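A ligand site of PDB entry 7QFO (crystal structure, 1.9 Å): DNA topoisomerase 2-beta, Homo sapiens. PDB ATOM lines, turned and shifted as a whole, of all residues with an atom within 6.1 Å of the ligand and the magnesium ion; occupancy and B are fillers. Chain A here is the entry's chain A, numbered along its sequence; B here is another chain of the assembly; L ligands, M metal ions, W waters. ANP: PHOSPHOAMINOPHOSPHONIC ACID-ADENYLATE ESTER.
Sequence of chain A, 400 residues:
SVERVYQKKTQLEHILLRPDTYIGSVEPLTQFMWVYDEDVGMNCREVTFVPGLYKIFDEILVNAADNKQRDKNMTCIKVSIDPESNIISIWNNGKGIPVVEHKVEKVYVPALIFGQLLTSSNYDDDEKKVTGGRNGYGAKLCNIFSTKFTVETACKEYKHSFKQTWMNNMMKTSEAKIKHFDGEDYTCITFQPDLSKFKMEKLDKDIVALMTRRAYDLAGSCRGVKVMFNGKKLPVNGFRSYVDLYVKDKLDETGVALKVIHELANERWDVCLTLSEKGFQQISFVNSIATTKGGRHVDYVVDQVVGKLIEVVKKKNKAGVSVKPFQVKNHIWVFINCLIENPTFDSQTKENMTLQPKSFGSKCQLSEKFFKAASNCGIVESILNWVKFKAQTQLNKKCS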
ATOM      1  N   GLU A  59     -28.554  21.653  11.474  1.00  0.00           N
ATOM      2  CA  GLU A  59     -27.446  20.644  11.400  1.00  0.00           C
ATOM      3  C   GLU A  59     -26.348  20.989  12.417  1.00  0.00           C
ATOM      4  O   GLU A  59     -25.817  20.047  13.082  1.00  0.00           O
ATOM      5  CB  GLU A  59     -26.866  20.562  10.003  1.00  0.00           C
ATOM      6  CG  GLU A  59     -27.791  19.969   8.968  1.00  0.00           C
ATOM      7  CD  GLU A  59     -28.097  18.489   9.093  1.00  0.00           C
ATOM      8  OE1 GLU A  59     -28.822  17.947   8.221  1.00  0.00           O
ATOM      9  OE2 GLU A  59     -27.610  17.863  10.083  1.00  0.00           O
ATOM     10  N   ILE A  60     -26.038  22.275  12.568  1.00  0.00           N
ATOM     11  CA  ILE A  60     -24.979  22.713  13.512  1.00  0.00           C
ATOM     12  C   ILE A  60     -25.514  22.637  14.935  1.00  0.00           C
ATOM     13  O   ILE A  60     -24.738  22.261  15.818  1.00  0.00           O
ATOM     14  CB  ILE A  60     -24.487  24.121  13.139  1.00  0.00           C
ATOM     15  CG1 ILE A  60     -24.058  24.214  11.677  1.00  0.00           C
ATOM     16  CG2 ILE A  60     -23.404  24.610  14.113  1.00  0.00           C
ATOM     17  CD1 ILE A  60     -23.022  23.185  11.273  1.00  0.00           C
ATOM     18  N   VAL A  62     -27.769  20.477  16.156  1.00  0.00           N
ATOM     19  CA  VAL A  62     -27.880  19.066  16.584  1.00  0.00           C
ATOM     20  C   VAL A  62     -26.448  18.522  16.810  1.00  0.00           C
ATOM     21  O   VAL A  62     -26.237  17.724  17.736  1.00  0.00           O
ATOM     22  CB  VAL A  62     -28.687  18.237  15.582  1.00  0.00           C
ATOM     23  CG1 VAL A  62     -28.574  16.759  15.855  1.00  0.00           C
ATOM     24  CG2 VAL A  62     -30.156  18.666  15.626  1.00  0.00           C
ATOM     25  N   ASN A  63     -25.492  18.983  16.021  1.00  0.00           N
ATOM     26  CA  ASN A  63     -24.074  18.598  16.223  1.00  0.00           C
ATOM     27  C   ASN A  63     -23.573  18.998  17.628  1.00  0.00           C
ATOM     28  O   ASN A  63     -22.904  18.169  18.234  1.00  0.00           O
ATOM     29  CB  ASN A  63     -23.169  19.196  15.186  1.00  0.00           C
ATOM     30  CG  ASN A  63     -23.196  18.457  13.885  1.00  0.00           C
ATOM     31  OD1 ASN A  63     -23.698  17.322  13.779  1.00  0.00           O
ATOM     32  ND2 ASN A  63     -22.671  19.142  12.872  1.00  0.00           N
ATOM     33  N   ALA A  64     -23.910  20.191  18.127  1.00  0.00           N
ATOM     34  CA  ALA A  64     -23.649  20.659  19.509  1.00  0.00           C
ATOM     35  C   ALA A  64     -24.313  19.731  20.524  1.00  0.00           C
ATOM     36  O   ALA A  64     -23.628  19.279  21.444  1.00  0.00           O
ATOM     37  CB  ALA A  64     -24.099  22.096  19.660  1.00  0.00           C
ATOM     38  N   ASP A  66     -25.184  16.684  20.067  1.00  0.00           N
ATOM     39  CA  ASP A  66     -24.511  15.375  19.936  1.00  0.00           C
ATOM     40  C   ASP A  66     -23.237  15.366  20.774  1.00  0.00           C
ATOM     41  O   ASP A  66     -22.842  14.268  21.185  1.00  0.00           O
ATOM     42  CB  ASP A  66     -24.195  15.011  18.486  1.00  0.00           C
ATOM     43  CG  ASP A  66     -25.415  14.597  17.691  1.00  0.00           C
ATOM     44  OD1 ASP A  66     -26.457  14.369  18.315  1.00  0.00           O
ATOM     45  OD2 ASP A  66     -25.281  14.455  16.429  1.00  0.00           O
ATOM     46  N   ASN A  67     -22.658  16.523  21.143  1.00  0.00           N
ATOM     47  CA  ASN A  67     -21.382  16.467  21.883  1.00  0.00           C
ATOM     48  C   ASN A  67     -21.642  16.020  23.319  1.00  0.00           C
ATOM     49  O   ASN A  67     -20.720  15.576  23.971  1.00  0.00           O
ATOM     50  CB  ASN A  67     -20.612  17.788  21.878  1.00  0.00           C
ATOM     51  CG  ASN A  67     -19.143  17.541  22.123  1.00  0.00           C
ATOM     52  OD1 ASN A  67     -18.501  16.822  21.344  1.00  0.00           O
ATOM     53  ND2 ASN A  67     -18.626  18.154  23.165  1.00  0.00           N
ATOM     54  N   ARG A  70     -20.597  12.477  23.355  1.00  0.00           N
ATOM     55  CA  ARG A  70     -19.132  12.247  23.358  1.00  0.00           C
ATOM     56  C   ARG A  70     -18.561  12.630  24.730  1.00  0.00           C
ATOM     57  O   ARG A  70     -17.448  12.231  24.994  1.00  0.00           O
ATOM     58  CB  ARG A  70     -18.381  13.131  22.359  1.00  0.00           C
ATOM     59  CG  ARG A  70     -18.445  12.701  20.906  1.00  0.00           C
ATOM     60  CD  ARG A  70     -17.597  13.670  20.096  1.00  0.00           C
ATOM     61  NE  ARG A  70     -16.157  13.596  20.407  1.00  0.00           N
ATOM     62  CZ  ARG A  70     -15.345  14.606  20.814  1.00  0.00           C
ATOM     63  NH1 ARG A  70     -15.777  15.852  20.989  1.00  0.00           N
ATOM     64  NH2 ARG A  70     -14.054  14.352  21.017  1.00  0.00           N
ATOM     65  N   ASN A  92     -20.281  25.273  22.020  1.00  0.00           N
ATOM     66  CA  ASN A  92     -20.540  24.245  23.035  1.00  0.00           C
ATOM     67  C   ASN A  92     -19.261  24.008  23.834  1.00  0.00           C
ATOM     68  O   ASN A  92     -18.168  24.127  23.260  1.00  0.00           O
ATOM     69  CB  ASN A  92     -21.068  22.964  22.395  1.00  0.00           C
ATOM     70  CG  ASN A  92     -20.061  22.241  21.519  1.00  0.00           C
ATOM     71  OD1 ASN A  92     -20.089  22.388  20.314  1.00  0.00           O
ATOM     72  ND2 ASN A  92     -19.223  21.404  22.112  1.00  0.00           N
ATOM     73  N   LYS A  95     -15.731  18.126  25.635  1.00  0.00           N
ATOM     74  CA  LYS A  95     -14.565  17.791  24.795  1.00  0.00           C
ATOM     75  C   LYS A  95     -14.644  18.442  23.427  1.00  0.00           C
ATOM     76  O   LYS A  95     -15.695  18.321  22.731  1.00  0.00           O
ATOM     77  CB  LYS A  95     -14.423  16.290  24.594  1.00  0.00           C
ATOM     78  CG  LYS A  95     -13.714  15.622  25.749  1.00  0.00           C
ATOM     79  CD  LYS A  95     -13.583  14.127  25.574  1.00  0.00           C
ATOM     80  CE  LYS A  95     -13.363  13.439  26.902  1.00  0.00           C
ATOM     81  NZ  LYS A  95     -13.036  12.013  26.728  1.00  0.00           N
ATOM     82  N   GLY A  96     -13.506  19.011  23.014  1.00  0.00           N
ATOM     83  CA  GLY A  96     -13.296  19.483  21.639  1.00  0.00           C
ATOM     84  C   GLY A  96     -12.964  18.346  20.698  1.00  0.00           C
ATOM     85  O   GLY A  96     -13.057  17.183  21.047  1.00  0.00           O
ATOM     86  N   ILE A  97     -12.611  18.688  19.474  1.00  0.00           N
ATOM     87  CA  ILE A  97     -12.258  17.699  18.426  1.00  0.00           C
ATOM     88  C   ILE A  97     -10.754  17.540  18.417  1.00  0.00           C
ATOM     89  O   ILE A  97     -10.042  18.550  18.422  1.00  0.00           O
ATOM     90  CB  ILE A  97     -12.773  18.227  17.079  1.00  0.00           C
ATOM     91  CG1 ILE A  97     -14.289  18.471  17.173  1.00  0.00           C
ATOM     92  CG2 ILE A  97     -12.420  17.271  15.966  1.00  0.00           C
ATOM     93  CD1 ILE A  97     -14.864  19.072  15.949  1.00  0.00           C
ATOM     94  N   ILE A 113     -13.527  16.535   8.722  1.00  0.00           N
ATOM     95  CA  ILE A 113     -14.939  16.229   9.104  1.00  0.00           C
ATOM     96  C   ILE A 113     -15.844  17.450   8.866  1.00  0.00           C
ATOM     97  O   ILE A 113     -17.073  17.263   8.938  1.00  0.00           O
ATOM     98  CB  ILE A 113     -15.006  15.671  10.531  1.00  0.00           C
ATOM     99  CG1 ILE A 113     -14.739  16.712  11.612  1.00  0.00           C
ATOM    100  CG2 ILE A 113     -14.133  14.424  10.639  1.00  0.00           C
ATOM    101  CD1 ILE A 113     -14.696  16.150  13.009  1.00  0.00           C
ATOM    102  N   PHE A 114     -15.273  18.636   8.618  1.00  0.00           N
ATOM    103  CA  PHE A 114     -16.015  19.874   8.267  1.00  0.00           C
ATOM    104  C   PHE A 114     -15.805  20.272   6.809  1.00  0.00           C
ATOM    105  O   PHE A 114     -16.617  21.077   6.326  1.00  0.00           O
ATOM    106  CB  PHE A 114     -15.630  21.014   9.206  1.00  0.00           C
ATOM    107  CG  PHE A 114     -16.241  20.886  10.564  1.00  0.00           C
ATOM    108  CD1 PHE A 114     -17.532  21.363  10.797  1.00  0.00           C
ATOM    109  CD2 PHE A 114     -15.522  20.358  11.619  1.00  0.00           C
ATOM    110  CE1 PHE A 114     -18.096  21.243  12.062  1.00  0.00           C
ATOM    111  CE2 PHE A 114     -16.069  20.260  12.886  1.00  0.00           C
ATOM    112  CZ  PHE A 114     -17.373  20.703  13.111  1.00  0.00           C
ATOM    113  N   THR A 119     -17.967  12.161   6.007  1.00  0.00           N
ATOM    114  CA  THR A 119     -17.033  12.035   7.142  1.00  0.00           C
ATOM    115  C   THR A 119     -17.804  12.169   8.453  1.00  0.00           C
ATOM    116  O   THR A 119     -18.600  13.105   8.560  1.00  0.00           O
ATOM    117  CB  THR A 119     -15.939  13.088   6.989  1.00  0.00           C
ATOM    118  OG1 THR A 119     -16.538  14.374   6.834  1.00  0.00           O
ATOM    119  CG2 THR A 119     -15.049  12.783   5.797  1.00  0.00           C
ATOM    120  N   SER A 120     -17.572  11.252   9.396  1.00  0.00           N
ATOM    121  CA  SER A 120     -18.370  11.077  10.640  1.00  0.00           C
ATOM    122  C   SER A 120     -17.626  10.211  11.670  1.00  0.00           C
ATOM    123  O   SER A 120     -16.816   9.345  11.283  1.00  0.00           O
ATOM    124  CB  SER A 120     -19.683  10.443  10.265  1.00  0.00           C
ATOM    125  OG  SER A 120     -20.628  10.469  11.314  1.00  0.00           O
ATOM    126  N   SER A 121     -17.963  10.428  12.925  1.00  0.00           N
ATOM    127  CA  SER A 121     -17.686   9.536  14.072  1.00  0.00           C
ATOM    128  C   SER A 121     -18.902   8.628  14.313  1.00  0.00           C
ATOM    129  O   SER A 121     -18.854   7.867  15.282  1.00  0.00           O
ATOM    130  CB  SER A 121     -17.339  10.344  15.281  1.00  0.00           C
ATOM    131  OG  SER A 121     -18.384  11.229  15.651  1.00  0.00           O
ATOM    132  N   ASN A 122     -19.931   8.704  13.464  1.00  0.00           N
ATOM    133  CA  ASN A 122     -21.195   7.950  13.634  1.00  0.00           C
ATOM    134  C   ASN A 122     -21.392   6.859  12.585  1.00  0.00           C
ATOM    135  O   ASN A 122     -22.549   6.435  12.425  1.00  0.00           O
ATOM    136  CB  ASN A 122     -22.377   8.920  13.608  1.00  0.00           C
ATOM    137  CG  ASN A 122     -22.355   9.828  14.807  1.00  0.00           C
ATOM    138  OD1 ASN A 122     -22.459   9.350  15.917  1.00  0.00           O
ATOM    139  ND2 ASN A 122     -22.278  11.129  14.584  1.00  0.00           N
ATOM    140  N   GLY A 132     -27.861  12.331  17.174  1.00  0.00           N
ATOM    141  CA  GLY A 132     -28.727  12.597  16.010  1.00  0.00           C
ATOM    142  C   GLY A 132     -27.966  12.376  14.729  1.00  0.00           C
ATOM    143  O   GLY A 132     -28.602  12.039  13.720  1.00  0.00           O
ATOM    144  N   GLY A 133     -26.643  12.603  14.788  1.00  0.00           N
ATOM    145  CA  GLY A 133     -25.782  12.466  13.607  1.00  0.00           C
ATOM    146  C   GLY A 133     -25.753  11.035  13.148  1.00  0.00           C
ATOM    147  O   GLY A 133     -25.551  10.132  13.996  1.00  0.00           O
ATOM    148  N   ARG A 134     -25.926  10.798  11.844  1.00  0.00           N
ATOM    149  CA  ARG A 134     -25.890   9.446  11.256  1.00  0.00           C
ATOM    150  C   ARG A 134     -25.097   9.421   9.960  1.00  0.00           C
ATOM    151  O   ARG A 134     -24.550   8.375   9.672  1.00  0.00           O
ATOM    152  CB  ARG A 134     -27.304   8.921  10.987  1.00  0.00           C
ATOM    153  CG  ARG A 134     -28.214   8.912  12.207  1.00  0.00           C
ATOM    154  CD  ARG A 134     -27.766   7.993  13.346  1.00  0.00           C
ATOM    155  NE  ARG A 134     -27.915   6.649  12.809  1.00  0.00           N
ATOM    156  CZ  ARG A 134     -27.045   5.650  12.919  1.00  0.00           C
ATOM    157  NH1 ARG A 134     -25.934   5.758  13.634  1.00  0.00           N
ATOM    158  NH2 ARG A 134     -27.323   4.520  12.305  1.00  0.00           N
ATOM    159  N   ASN A 135     -25.097  10.475   9.150  1.00  0.00           N
ATOM    160  CA  ASN A 135     -24.802  10.310   7.707  1.00  0.00           C
ATOM    161  C   ASN A 135     -23.449  10.896   7.294  1.00  0.00           C
ATOM    162  O   ASN A 135     -23.033  10.605   6.138  1.00  0.00           O
ATOM    163  CB  ASN A 135     -25.902  10.919   6.846  1.00  0.00           C
ATOM    164  CG  ASN A 135     -27.237  10.251   7.108  1.00  0.00           C
ATOM    165  OD1 ASN A 135     -27.288   9.047   7.340  1.00  0.00           O
ATOM    166  ND2 ASN A 135     -28.275  11.041   7.169  1.00  0.00           N
ATOM    167  N   GLY A 136     -22.860  11.785   8.084  1.00  0.00           N
ATOM    168  CA  GLY A 136     -21.597  12.443   7.680  1.00  0.00           C
ATOM    169  C   GLY A 136     -21.781  13.541   6.633  1.00  0.00           C
ATOM    170  O   GLY A 136     -20.842  13.792   5.879  1.00  0.00           O
ATOM    171  N   TYR A 137     -22.942  14.194   6.586  1.00  0.00           N
ATOM    172  CA  TYR A 137     -23.192  15.351   5.686  1.00  0.00           C
ATOM    173  C   TYR A 137     -23.340  16.706   6.415  1.00  0.00           C
ATOM    174  O   TYR A 137     -22.927  17.730   5.860  1.00  0.00           O
ATOM    175  CB  TYR A 137     -24.463  15.124   4.898  1.00  0.00           C
ATOM    176  CG  TYR A 137     -24.282  14.368   3.625  1.00  0.00           C
ATOM    177  CD1 TYR A 137     -23.546  14.911   2.595  1.00  0.00           C
ATOM    178  CD2 TYR A 137     -24.963  13.181   3.387  1.00  0.00           C
ATOM    179  CE1 TYR A 137     -23.424  14.253   1.383  1.00  0.00           C
ATOM    180  CE2 TYR A 137     -24.872  12.522   2.173  1.00  0.00           C
ATOM    181  CZ  TYR A 137     -24.071  13.054   1.174  1.00  0.00           C
ATOM    182  OH  TYR A 137     -23.943  12.484  -0.058  1.00  0.00           O
ATOM    183  N   GLY A 138     -24.037  16.742   7.548  1.00  0.00           N
ATOM    184  CA  GLY A 138     -24.681  17.963   8.073  1.00  0.00           C
ATOM    185  C   GLY A 138     -23.785  19.192   8.057  1.00  0.00           C
ATOM    186  O   GLY A 138     -24.217  20.285   7.632  1.00  0.00           O
ATOM    187  N   ALA A 139     -22.604  19.081   8.646  1.00  0.00           N
ATOM    188  CA  ALA A 139     -21.705  20.228   8.787  1.00  0.00           C
ATOM    189  C   ALA A 139     -21.234  20.690   7.416  1.00  0.00           C
ATOM    190  O   ALA A 139     -21.118  21.903   7.210  1.00  0.00           O
ATOM    191  CB  ALA A 139     -20.568  19.930   9.719  1.00  0.00           C
ATOM    192  N   LYS A 140     -20.929  19.771   6.519  1.00  0.00           N
ATOM    193  CA  LYS A 140     -20.451  20.134   5.166  1.00  0.00           C
ATOM    194  C   LYS A 140     -21.593  20.838   4.429  1.00  0.00           C
ATOM    195  O   LYS A 140     -21.305  21.788   3.694  1.00  0.00           O
ATOM    196  CB  LYS A 140     -19.987  18.889   4.422  1.00  0.00           C
ATOM    197  CG  LYS A 140     -18.563  18.424   4.748  1.00  0.00           C
ATOM    198  CD  LYS A 140     -18.412  17.773   6.070  1.00  0.00           C
ATOM    199  CE  LYS A 140     -19.106  16.435   6.191  1.00  0.00           C
ATOM    200  NZ  LYS A 140     -18.961  15.858   7.557  1.00  0.00           N
ATOM    201  N   THR A 153     -12.049  24.923  17.473  1.00  0.00           N
ATOM    202  CA  THR A 153     -12.146  23.837  18.484  1.00  0.00           C
ATOM    203  C   THR A 153     -10.851  23.823  19.299  1.00  0.00           C
ATOM    204  O   THR A 153      -9.793  24.116  18.721  1.00  0.00           O
ATOM    205  CB  THR A 153     -12.524  22.519  17.807  1.00  0.00           C
ATOM    206  OG1 THR A 153     -12.906  21.600  18.819  1.00  0.00           O
ATOM    207  CG2 THR A 153     -11.447  21.913  16.931  1.00  0.00           C
ATOM    208  N   THR A 187     -16.020  23.875  21.235  1.00  0.00           N
ATOM    209  CA  THR A 187     -16.143  24.033  19.773  1.00  0.00           C
ATOM    210  C   THR A 187     -17.081  25.212  19.497  1.00  0.00           C
ATOM    211  O   THR A 187     -18.140  25.352  20.142  1.00  0.00           O
ATOM    212  CB  THR A 187     -16.588  22.724  19.098  1.00  0.00           C
ATOM    213  OG1 THR A 187     -15.654  21.696  19.356  1.00  0.00           O
ATOM    214  CG2 THR A 187     -16.695  22.818  17.592  1.00  0.00           C
ATOM    215  N   ILE A 189     -18.826  27.005  16.020  1.00  0.00           N
ATOM    216  CA  ILE A 189     -19.037  27.088  14.561  1.00  0.00           C
ATOM    217  C   ILE A 189     -19.671  28.458  14.301  1.00  0.00           C
ATOM    218  O   ILE A 189     -20.752  28.741  14.866  1.00  0.00           O
ATOM    219  CB  ILE A 189     -19.907  25.925  14.055  1.00  0.00           C
ATOM    220  CG1 ILE A 189     -19.354  24.545  14.440  1.00  0.00           C
ATOM    221  CG2 ILE A 189     -20.148  26.071  12.567  1.00  0.00           C
ATOM    222  CD1 ILE A 189     -17.906  24.303  14.057  1.00  0.00           C
ATOM    223  N   GLN A 348     -32.106  13.148   4.641  1.00  0.00           N
ATOM    224  CA  GLN A 348     -31.073  13.898   5.402  1.00  0.00           C
ATOM    225  C   GLN A 348     -31.745  14.869   6.384  1.00  0.00           C
ATOM    226  O   GLN A 348     -31.159  15.124   7.437  1.00  0.00           O
ATOM    227  CB  GLN A 348     -30.062  14.617   4.492  1.00  0.00           C
ATOM    228  CG  GLN A 348     -29.052  15.451   5.256  1.00  0.00           C
ATOM    229  CD  GLN A 348     -28.110  14.631   6.125  1.00  0.00           C
ATOM    230  OE1 GLN A 348     -27.799  13.484   5.839  1.00  0.00           O
ATOM    231  NE2 GLN A 348     -27.647  15.211   7.208  1.00  0.00           N
ATOM    232  N   LYS A 350     -34.365  14.460   8.249  1.00  0.00           N
ATOM    233  CA  LYS A 350     -34.696  13.713   9.508  1.00  0.00           C
ATOM    234  C   LYS A 350     -36.017  14.185  10.145  1.00  0.00           C
ATOM    235  O   LYS A 350     -36.149  14.180  11.400  1.00  0.00           O
ATOM    236  CB  LYS A 350     -33.516  13.888  10.460  1.00  0.00           C
ATOM    237  CG  LYS A 350     -32.272  13.123  10.012  1.00  0.00           C
ATOM    238  CD  LYS A 350     -31.159  13.336  10.958  1.00  0.00           C
ATOM    239  CE  LYS A 350     -29.787  13.141  10.340  1.00  0.00           C
ATOM    240  NZ  LYS A 350     -28.755  13.600  11.289  1.00  0.00           N
ATOM    241  N   TYR B   6     -13.015   8.683  13.560  1.00  0.00           N
ATOM    242  CA  TYR B   6     -13.314   9.574  12.415  1.00  0.00           C
ATOM    243  C   TYR B   6     -13.041   8.846  11.119  1.00  0.00           C
ATOM    244  O   TYR B   6     -11.857   8.529  10.798  1.00  0.00           O
ATOM    245  CB  TYR B   6     -12.536  10.876  12.531  1.00  0.00           C
ATOM    246  CG  TYR B   6     -12.837  11.590  13.818  1.00  0.00           C
ATOM    247  CD1 TYR B   6     -13.975  12.373  13.939  1.00  0.00           C
ATOM    248  CD2 TYR B   6     -12.031  11.433  14.928  1.00  0.00           C
ATOM    249  CE1 TYR B   6     -14.269  13.028  15.121  1.00  0.00           C
ATOM    250  CE2 TYR B   6     -12.293  12.080  16.116  1.00  0.00           C
ATOM    251  CZ  TYR B   6     -13.419  12.865  16.207  1.00  0.00           C
ATOM    252  OH  TYR B   6     -13.710  13.483  17.367  1.00  0.00           O
HETATM  253  PG  ANP L   1     -25.254  13.931   9.939  1.00  0.00           P
HETATM  254  O1G ANP L   1     -26.418  12.930   9.948  1.00  0.00           O
HETATM  255  O2G ANP L   1     -24.956  14.186   8.479  1.00  0.00           O
HETATM  256  O3G ANP L   1     -25.344  15.173  10.701  1.00  0.00           O
HETATM  257  PB  ANP L   1     -22.761  13.709  11.555  1.00  0.00           P
HETATM  258  O1B ANP L   1     -23.192  14.631  12.631  1.00  0.00           O
HETATM  259  O2B ANP L   1     -21.862  12.573  11.994  1.00  0.00           O
HETATM  260  N3B ANP L   1     -23.964  13.084  10.630  1.00  0.00           N
HETATM  261  PA  ANP L   1     -21.626  16.130  10.405  1.00  0.00           P
HETATM  262  O1A ANP L   1     -21.138  16.440   9.047  1.00  0.00           O
HETATM  263  O2A ANP L   1     -22.805  16.924  10.953  1.00  0.00           O
HETATM  264  O3A ANP L   1     -21.946  14.581  10.508  1.00  0.00           O
HETATM  265  O5' ANP L   1     -20.445  16.300  11.493  1.00  0.00           O
HETATM  266  C5' ANP L   1     -19.207  15.630  11.164  1.00  0.00           C
HETATM  267  C4' ANP L   1     -18.546  15.137  12.431  1.00  0.00           C
HETATM  268  O4' ANP L   1     -17.919  16.263  13.098  1.00  0.00           O
HETATM  269  C3' ANP L   1     -19.417  14.473  13.489  1.00  0.00           C
HETATM  270  O3' ANP L   1     -19.495  13.073  13.233  1.00  0.00           O
HETATM  271  C2' ANP L   1     -18.628  14.743  14.762  1.00  0.00           C
HETATM  272  O2' ANP L   1     -17.611  13.775  14.928  1.00  0.00           O
HETATM  273  C1' ANP L   1     -17.972  16.090  14.487  1.00  0.00           C
HETATM  274  N9  ANP L   1     -18.585  17.253  15.064  1.00  0.00           N
HETATM  275  C8  ANP L   1     -19.461  18.168  14.456  1.00  0.00           C
HETATM  276  N7  ANP L   1     -19.817  19.126  15.276  1.00  0.00           N
HETATM  277  C5  ANP L   1     -19.133  18.860  16.461  1.00  0.00           C
HETATM  278  C6  ANP L   1     -19.130  19.495  17.723  1.00  0.00           C
HETATM  279  N6  ANP L   1     -19.842  20.581  18.029  1.00  0.00           N
HETATM  280  N1  ANP L   1     -18.337  18.968  18.698  1.00  0.00           N
HETATM  281  C2  ANP L   1     -17.650  17.845  18.413  1.00  0.00           C
HETATM  282  N3  ANP L   1     -17.577  17.164  17.275  1.00  0.00           N
HETATM  283  C4  ANP L   1     -18.368  17.722  16.338  1.00  0.00           C
HETATM  284 MG    MG M   1     -24.379  16.233  12.149  1.00  0.00          MG
HETATM  285  O   HOH W   1     -16.015  14.850  17.645  1.00  0.00           O
HETATM  286  O   HOH W   2     -21.211  16.298  17.057  1.00  0.00           O
HETATM  287  O   HOH W   3     -25.522  18.076  11.634  1.00  0.00           O
HETATM  288  O   HOH W   4     -20.974  21.334  13.933  1.00  0.00           O
HETATM  289  O   HOH W   5     -16.981  20.023  20.991  1.00  0.00           O
HETATM  290  O   HOH W   6     -22.731  14.718  15.444  1.00  0.00           O
HETATM  291  O   HOH W   7     -19.729  15.351  19.069  1.00  0.00           O
HETATM  292  O   HOH W   8     -21.898  22.372  16.446  1.00  0.00           O
HETATM  293  O   HOH W   9     -25.984  15.727  13.574  1.00  0.00           O
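The side-chain hydroxyl (OG) of Ser 120 is in hydrogen-bond range of an oxygen (O2B) of the ligand (2.5 Å).
An oxygen (O1A) of the ligand is in salt-bridge range of the side-chain amino group of Lys 140, at 2.7 Å.
O3' of the ligand lies within hydrogen-bond range of N of Ser 121, 3.1 Å away.
The side-chain hydroxyl of Ser 121 lies within hydrogen-bond range of an oxygen (O2') of the ligand (2.8 Å).
The backbone NH (N) of Tyr 137 sits at hydrogen-bond distance from an oxygen (O2G) of the ligand (2.8 Å).
The side-chain amino group (NZ) of Lys 350 is in salt-bridge range of an oxygen (O1G) of the ligand, 2.8 Å away.
The backbone NH (N) of Gly 138 is in hydrogen-bond range of an oxygen (O2G) of the ligand (2.9 Å).
N of Arg 134 sits at hydrogen-bond distance from O1G of the ligand, at 2.9 Å.
O1G of the ligand lies within hydrogen-bond range of N of Asn 135, at 2.9 Å.
The side-chain amide oxygen (OD1) of Asn 92 sits at hydrogen-bond distance from a nitrogen (N6) of the ligand (2.9 Å).
An oxygen (O2B) of the ligand sits at hydrogen-bond distance from the side-chain amide nitrogen (ND2) of Asn 122.
The backbone NH of Ala 139 sits at hydrogen-bond distance from an oxygen (O1A) of the ligand (3.0 Å).
The backbone NH (N) of Gly 136 lies within hydrogen-bond range of an oxygen (O2G) of the ligand (3.2 Å).
The side-chain amide nitrogen (NE2) of Gln 348 sits at hydrogen-bond distance from an oxygen (O2G) of the ligand, at 3.1 Å.
OD1 of Asn 67 sits close to N1 of the ligand (3.4 Å).
Within 4 Å of the magnesium ion: Asn 63.
The side-chain hydroxyl of Ser 120 lies within hydrogen-bond range of the backbone NH of Asn 122.
The side-chain amino group (NZ) of Lys 140 sits close to the backbone carbonyl oxygen (O) of Gly 136.
The side-chain amino group (NZ) of Lys 350 is in hydrogen-bond range of the backbone carbonyl oxygen (O) of Gly 132, at 2.9 Å.
ND2 of Asn 92 sits close to ND2 of Asn 67, at 3.5 Å.
O of Gly 133 lies close to ND2 of Asn 122 (3.5 Å).
The backbone NH (N) of Ile 97 is in hydrogen-bond range of the side-chain hydroxyl (OG1) of Thr 153 (3.0 Å).
The guanidinium group (NH2) of Arg 70 sits at hydrogen-bond distance from the backbone carbonyl oxygen (O) of Gly 96.
The side-chain hydroxyl (OG1) of Thr 187 is in hydrogen-bond range of the side-chain hydroxyl (OG1) of Thr 153, 2.8 Å away.
Merely in contact with the ligand: Ile 113 (3.2 Å), Tyr 6 of chain B (3.4 Å), Gly 133 (3.5 Å), Ile 97 (3.5 Å), Phe 114 (3.5 Å), Glu 59 (3.6 Å), Thr 119 (3.7 Å), Arg 70 (3.8 Å) and Thr 187 (3.9 Å).
Hydrophobic or aromatic side chains that line the ligand: Ile 97, Ile 113, Phe 114, Tyr 137, Ala 139 and Tyr 6 of chain B.
Of the 33 residues printed, 24 come within 4 Å of the ligand.
Along chain A the residues within 4 Å of the ligand span positions 59 to 350.
Water W3 bridges O of Glu 59 and ND2 of Asn 63.
Water W9 lies within hydrogen-bond range of the side-chain carboxylate (OD2) of Asp 66 (3.2 Å) and the backbone NH (N) of Gly 133 (3.4 Å).
Water W1 lies within hydrogen-bond range of the side-chain hydroxyl (OH) of Tyr 6 of chain B, a nitrogen (N3) of the ligand and the guanidinium group (NE) of Arg 70.
Water W4 bridges a nitrogen (N7) of the ligand (2.8 Å) and the side-chain amide nitrogen (ND2) of Asn 63 (3.0 Å).
Water W8 lies within hydrogen-bond range of O of Ile 60 (2.9 Å), N6 of the ligand (3.2 Å) and N of Ala 64 (3.4 Å).
Water W7 lies within hydrogen-bond range of the side-chain amide oxygen of Asn 67 (3.0 Å) and a nitrogen (N3) of the ligand (3.3 Å).
The magnesium ion is bound by O3G of the ligand, O1B of the ligand, OD1 of Asn 63, O2A of the ligand, water W9 and water W3.
The magnesium ion has six donor atoms within binding distance.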
